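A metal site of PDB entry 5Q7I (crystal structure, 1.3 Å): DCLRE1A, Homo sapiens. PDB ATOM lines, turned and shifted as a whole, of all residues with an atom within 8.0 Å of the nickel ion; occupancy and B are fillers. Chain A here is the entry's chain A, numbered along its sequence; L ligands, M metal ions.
The side-chain carboxylate (OD2) of Asp 118 sits close to a ring nitrogen (NE2) of His 40 (3.3 Å).
The backbone carbonyl oxygen (O) of Ile 184 lies within hydrogen-bond range of a ring nitrogen (NE2) of His 37, 2.9 Å away.
A ring nitrogen (ND1) of His 35 sits at hydrogen-bond distance from the side-chain hydroxyl (OG1) of Thr 34 (2.9 Å).
ND1 of His 96 lies within hydrogen-bond range of O of Glu 296 (2.8 Å).
Within 4 Å of the nickel ion: His 35, His 37, His 96 and Asp 118.
The nickel ion is bound by an oxygen (O3) of the ligand (2.0 Å), an oxygen (O2) of the ligand (2.2 Å), the side-chain carboxylate (OD2) of Asp 118 (2.2 Å), a ring nitrogen (ND1) of His 37 (2.2 Å), a ring nitrogen (NE2) of His 35 (2.3 Å) and a ring nitrogen (NE2) of His 96 (2.3 Å).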
ATOM      1  N   ASP A  18      15.340   9.777   7.618  1.00  0.00           N
ATOM      2  CA  ASP A  18      15.815   9.666   9.033  1.00  0.00           C
ATOM      3  C   ASP A  18      17.302  10.201   9.204  1.00  0.00           C
ATOM      4  O   ASP A  18      18.115   9.574   9.920  1.00  0.00           O
ATOM      5  CB  ASP A  18      15.573   8.296   9.627  1.00  0.00           C
ATOM      6  CG  ASP A  18      14.064   7.856   9.576  1.00  0.00           C
ATOM      7  OD1 ASP A  18      13.225   8.766   9.355  1.00  0.00           O
ATOM      8  OD2 ASP A  18      13.865   6.651   9.832  1.00  0.00           O
ATOM      9  N   THR A  34      10.407   8.779   9.193  1.00  0.00           N
ATOM     10  CA  THR A  34       9.500   7.597   9.224  1.00  0.00           C
ATOM     11  C   THR A  34       8.635   7.525  10.508  1.00  0.00           C
ATOM     12  O   THR A  34       7.491   7.074  10.425  1.00  0.00           O
ATOM     13  CB  THR A  34      10.261   6.279   9.009  1.00  0.00           C
ATOM     14  OG1 THR A  34      11.198   6.069  10.126  1.00  0.00           O
ATOM     15  CG2 THR A  34      11.005   6.222   7.675  1.00  0.00           C
ATOM     16  N   HIS A  35       9.210   7.950  11.654  1.00  0.00           N
ATOM     17  CA  HIS A  35       8.484   7.866  12.934  1.00  0.00           C
ATOM     18  C   HIS A  35       9.179   8.667  13.974  1.00  0.00           C
ATOM     19  O   HIS A  35      10.396   8.952  13.867  1.00  0.00           O
ATOM     20  CB  HIS A  35       8.285   6.366  13.359  1.00  0.00           C
ATOM     21  CG  HIS A  35       9.522   5.615  13.724  1.00  0.00           C
ATOM     22  ND1 HIS A  35      10.507   5.237  12.849  1.00  0.00           N
ATOM     23  CD2 HIS A  35       9.877   5.062  14.900  1.00  0.00           C
ATOM     24  CE1 HIS A  35      11.415   4.496  13.498  1.00  0.00           C
ATOM     25  NE2 HIS A  35      11.018   4.387  14.739  1.00  0.00           N
ATOM     26  N   PHE A  36       8.431   8.947  15.042  1.00  0.00           N
ATOM     27  CA  PHE A  36       8.991   9.768  16.197  1.00  0.00           C
ATOM     28  C   PHE A  36       9.650   8.943  17.266  1.00  0.00           C
ATOM     29  O   PHE A  36       9.109   8.833  18.424  1.00  0.00           O
ATOM     30  CB  PHE A  36       7.819  10.591  16.773  1.00  0.00           C
ATOM     31  CG  PHE A  36       8.230  11.745  17.692  1.00  0.00           C
ATOM     32  CD1 PHE A  36       8.779  12.901  17.127  1.00  0.00           C
ATOM     33  CD2 PHE A  36       8.107  11.671  19.058  1.00  0.00           C
ATOM     34  CE1 PHE A  36       9.147  14.004  17.946  1.00  0.00           C
ATOM     35  CE2 PHE A  36       8.474  12.748  19.894  1.00  0.00           C
ATOM     36  CZ  PHE A  36       8.956  13.885  19.340  1.00  0.00           C
ATOM     37  N   HIS A  37      10.826   8.332  16.956  1.00  0.00           N
ATOM     38  CA  HIS A  37      11.750   7.691  17.892  1.00  0.00           C
ATOM     39  C   HIS A  37      13.073   8.448  17.802  1.00  0.00           C
ATOM     40  O   HIS A  37      13.554   8.765  16.700  1.00  0.00           O
ATOM     41  CB  HIS A  37      11.947   6.170  17.680  1.00  0.00           C
ATOM     42  CG  HIS A  37      10.841   5.287  18.233  1.00  0.00           C
ATOM     43  ND1 HIS A  37      10.638   3.969  17.848  1.00  0.00           N
ATOM     44  CD2 HIS A  37       9.892   5.549  19.155  1.00  0.00           C
ATOM     45  CE1 HIS A  37       9.648   3.435  18.555  1.00  0.00           C
ATOM     46  NE2 HIS A  37       9.160   4.395  19.335  1.00  0.00           N
ATOM     47  N   SER A  38      13.698   8.660  18.973  1.00  0.00           N
ATOM     48  CA  SER A  38      14.853   9.587  19.106  1.00  0.00           C
ATOM     49  C   SER A  38      16.015   9.197  18.221  1.00  0.00           C
ATOM     50  O   SER A  38      16.634  10.156  17.674  1.00  0.00           O
ATOM     51  CB  SER A  38      15.186   9.861  20.596  1.00  0.00           C
ATOM     52  OG  SER A  38      15.607   8.655  21.191  1.00  0.00           O
ATOM     53  N   ASP A  39      16.335   7.911  18.039  1.00  0.00           N
ATOM     54  CA  ASP A  39      17.489   7.525  17.142  1.00  0.00           C
ATOM     55  C   ASP A  39      17.228   8.019  15.710  1.00  0.00           C
ATOM     56  O   ASP A  39      18.173   8.254  14.916  1.00  0.00           O
ATOM     57  CB  ASP A  39      17.798   6.041  17.112  1.00  0.00           C
ATOM     58  CG  ASP A  39      18.595   5.535  18.380  1.00  0.00           C
ATOM     59  OD1 ASP A  39      18.959   6.384  19.219  1.00  0.00           O
ATOM     60  OD2 ASP A  39      18.749   4.299  18.444  1.00  0.00           O
ATOM     61  N   HIS A  40      15.940   8.172  15.307  1.00  0.00           N
ATOM     62  CA  HIS A  40      15.563   8.565  13.951  1.00  0.00           C
ATOM     63  C   HIS A  40      15.364  10.025  13.769  1.00  0.00           C
ATOM     64  O   HIS A  40      15.752  10.610  12.702  1.00  0.00           O
ATOM     65  CB  HIS A  40      14.269   7.727  13.562  1.00  0.00           C
ATOM     66  CG  HIS A  40      14.510   6.282  13.534  1.00  0.00           C
ATOM     67  ND1 HIS A  40      14.710   5.545  12.365  1.00  0.00           N
ATOM     68  CD2 HIS A  40      14.621   5.369  14.545  1.00  0.00           C
ATOM     69  CE1 HIS A  40      14.952   4.290  12.677  1.00  0.00           C
ATOM     70  NE2 HIS A  40      14.916   4.172  14.002  1.00  0.00           N
ATOM     71  N   HIS A  96       4.373  -0.354  13.571  1.00  0.00           N
ATOM     72  CA  HIS A  96       5.483  -0.065  14.560  1.00  0.00           C
ATOM     73  C   HIS A  96       4.805   0.706  15.666  1.00  0.00           C
ATOM     74  O   HIS A  96       3.924   0.089  16.332  1.00  0.00           O
ATOM     75  CB  HIS A  96       6.696   0.585  13.889  1.00  0.00           C
ATOM     76  CG  HIS A  96       7.920   0.827  14.725  1.00  0.00           C
ATOM     77  ND1 HIS A  96       8.473  -0.149  15.488  1.00  0.00           N
ATOM     78  CD2 HIS A  96       8.601   1.954  14.988  1.00  0.00           C
ATOM     79  CE1 HIS A  96       9.538   0.353  16.132  1.00  0.00           C
ATOM     80  NE2 HIS A  96       9.656   1.635  15.829  1.00  0.00           N
ATOM     81  N   CYS A  97       5.182   1.926  15.948  1.00  0.00           N
ATOM     82  CA  CYS A  97       4.484   2.822  16.966  1.00  0.00           C
ATOM     83  C   CYS A  97       3.465   3.741  16.251  1.00  0.00           C
ATOM     84  O   CYS A  97       3.458   3.808  15.006  1.00  0.00           O
ATOM     85  CB  CYS A  97       5.594   3.643  17.687  1.00  0.00           C
ATOM     86  SG  CYS A  97       6.535   4.804  16.583  1.00  0.00           S
ATOM     87  N   ALA A 100       4.010   5.717  12.600  1.00  0.00           N
ATOM     88  CA  ALA A 100       5.165   5.121  11.862  1.00  0.00           C
ATOM     89  C   ALA A 100       4.739   4.677  10.490  1.00  0.00           C
ATOM     90  O   ALA A 100       3.711   4.007  10.338  1.00  0.00           O
ATOM     91  CB  ALA A 100       5.779   3.984  12.641  1.00  0.00           C
ATOM     92  N   GLY A 117      11.324   1.918   7.054  1.00  0.00           N
ATOM     93  CA  GLY A 117      11.530   2.513   8.368  1.00  0.00           C
ATOM     94  C   GLY A 117      11.719   1.408   9.376  1.00  0.00           C
ATOM     95  O   GLY A 117      12.334   0.382   9.073  1.00  0.00           O
ATOM     96  N   ASP A 118      11.254   1.600  10.604  1.00  0.00           N
ATOM     97  CA  ASP A 118      11.079   0.504  11.565  1.00  0.00           C
ATOM     98  C   ASP A 118       9.683  -0.119  11.345  1.00  0.00           C
ATOM     99  O   ASP A 118       8.670   0.593  11.216  1.00  0.00           O
ATOM    100  CB  ASP A 118      11.196   0.957  13.019  1.00  0.00           C
ATOM    101  CG  ASP A 118      12.621   1.241  13.521  1.00  0.00           C
ATOM    102  OD1 ASP A 118      13.596   0.881  12.811  1.00  0.00           O
ATOM    103  OD2 ASP A 118      12.783   1.714  14.679  1.00  0.00           O
ATOM    104  N   PHE A 119       9.605  -1.447  11.327  1.00  0.00           N
ATOM    105  CA  PHE A 119       8.320  -2.147  11.059  1.00  0.00           C
ATOM    106  C   PHE A 119       8.218  -3.508  11.740  1.00  0.00           C
ATOM    107  O   PHE A 119       9.216  -4.102  12.061  1.00  0.00           O
ATOM    108  CB  PHE A 119       7.994  -2.234   9.510  1.00  0.00           C
ATOM    109  CG  PHE A 119       8.549  -3.429   8.704  1.00  0.00           C
ATOM    110  CD1 PHE A 119       7.771  -4.065   7.723  1.00  0.00           C
ATOM    111  CD2 PHE A 119       9.856  -3.879   8.869  1.00  0.00           C
ATOM    112  CE1 PHE A 119       8.276  -5.075   6.935  1.00  0.00           C
ATOM    113  CE2 PHE A 119      10.371  -4.932   8.113  1.00  0.00           C
ATOM    114  CZ  PHE A 119       9.555  -5.511   7.155  1.00  0.00           C
ATOM    115  N   ASP A 141      14.339  -2.872   7.781  1.00  0.00           N
ATOM    116  CA  ASP A 141      14.578  -2.960   9.279  1.00  0.00           C
ATOM    117  C   ASP A 141      14.926  -4.416   9.586  1.00  0.00           C
ATOM    118  O   ASP A 141      14.061  -5.301   9.663  1.00  0.00           O
ATOM    119  CB  ASP A 141      13.312  -2.513  10.006  1.00  0.00           C
ATOM    120  CG  ASP A 141      13.318  -2.831  11.493  1.00  0.00           C
ATOM    121  OD1 ASP A 141      14.429  -3.116  12.025  1.00  0.00           O
ATOM    122  OD2 ASP A 141      12.225  -2.735  12.076  1.00  0.00           O
ATOM    123  N   THR A 143      16.439  -5.393  12.544  1.00  0.00           N
ATOM    124  CA  THR A 143      16.709  -5.470  13.992  1.00  0.00           C
ATOM    125  C   THR A 143      16.841  -6.875  14.498  1.00  0.00           C
ATOM    126  O   THR A 143      17.887  -7.180  15.168  1.00  0.00           O
ATOM    127  CB  THR A 143      15.572  -4.717  14.766  1.00  0.00           C
ATOM    128  OG1 THR A 143      15.530  -3.335  14.455  1.00  0.00           O
ATOM    129  CG2 THR A 143      15.737  -4.882  16.278  1.00  0.00           C
ATOM    130  N   SER A 183       9.296   6.052  25.447  1.00  0.00           N
ATOM    131  CA  SER A 183       9.131   6.505  24.081  1.00  0.00           C
ATOM    132  C   SER A 183       7.631   6.246  23.761  1.00  0.00           C
ATOM    133  O   SER A 183       6.949   5.495  24.521  1.00  0.00           O
ATOM    134  CB  SER A 183       9.977   5.701  23.051  1.00  0.00           C
ATOM    135  OG  SER A 183       9.739   4.322  23.175  1.00  0.00           O
ATOM    136  N   ILE A 184       7.178   6.691  22.623  1.00  0.00           N
ATOM    137  CA  ILE A 184       5.876   6.254  22.118  1.00  0.00           C
ATOM    138  C   ILE A 184       5.975   4.812  21.639  1.00  0.00           C
ATOM    139  O   ILE A 184       7.109   4.285  21.347  1.00  0.00           O
ATOM    140  CB  ILE A 184       5.316   7.186  21.012  1.00  0.00           C
ATOM    141  CG1 ILE A 184       6.135   7.177  19.732  1.00  0.00           C
ATOM    142  CG2 ILE A 184       5.038   8.606  21.552  1.00  0.00           C
ATOM    143  CD1 ILE A 184       5.472   7.782  18.531  1.00  0.00           C
ATOM    144  N   GLU A 296       7.508  -4.391  18.782  1.00  0.00           N
ATOM    145  CA  GLU A 296       7.046  -3.604  17.598  1.00  0.00           C
ATOM    146  C   GLU A 296       8.001  -3.707  16.377  1.00  0.00           C
ATOM    147  O   GLU A 296       8.014  -2.884  15.451  1.00  0.00           O
ATOM    148  CB  GLU A 296       6.683  -2.170  17.963  1.00  0.00           C
ATOM    149  CG  GLU A 296       5.391  -2.109  18.873  1.00  0.00           C
ATOM    150  CD  GLU A 296       4.853  -0.730  19.209  1.00  0.00           C
ATOM    151  OE1 GLU A 296       5.638   0.285  19.125  1.00  0.00           O
ATOM    152  OE2 GLU A 296       3.637  -0.635  19.585  1.00  0.00           O
ATOM    153  N   HIS A 297       8.870  -4.744  16.455  1.00  0.00           N
ATOM    154  CA  HIS A 297       9.718  -5.117  15.271  1.00  0.00           C
ATOM    155  C   HIS A 297       9.426  -6.568  14.790  1.00  0.00           C
ATOM    156  O   HIS A 297       9.034  -7.430  15.629  1.00  0.00           O
ATOM    157  CB  HIS A 297      11.257  -5.016  15.604  1.00  0.00           C
ATOM    158  CG  HIS A 297      11.753  -3.645  15.901  1.00  0.00           C
ATOM    159  ND1 HIS A 297      12.183  -2.771  14.913  1.00  0.00           N
ATOM    160  CD2 HIS A 297      12.012  -3.027  17.103  1.00  0.00           C
ATOM    161  CE1 HIS A 297      12.629  -1.672  15.501  1.00  0.00           C
ATOM    162  NE2 HIS A 297      12.482  -1.795  16.799  1.00  0.00           N
HETATM  163  C1  LIG L   1      13.617   2.359  18.836  1.00  0.00           C
HETATM  164  C2  LIG L   1      12.976   1.052  18.417  1.00  0.00           C
HETATM  165  C3  LIG L   1      14.197   3.170  17.651  1.00  0.00           C
HETATM  166  O1  LIG L   1      13.254  -0.066  18.894  1.00  0.00           O
HETATM  167  O2  LIG L   1      12.140   1.132  17.567  1.00  0.00           O
HETATM  168  O3  LIG L   1      13.456   3.480  16.692  1.00  0.00           O
HETATM  169  O4  LIG L   1      15.395   3.596  17.778  1.00  0.00           O
HETATM  170 NI    NI M   1      11.603   2.772  16.206  1.00  0.00          NI
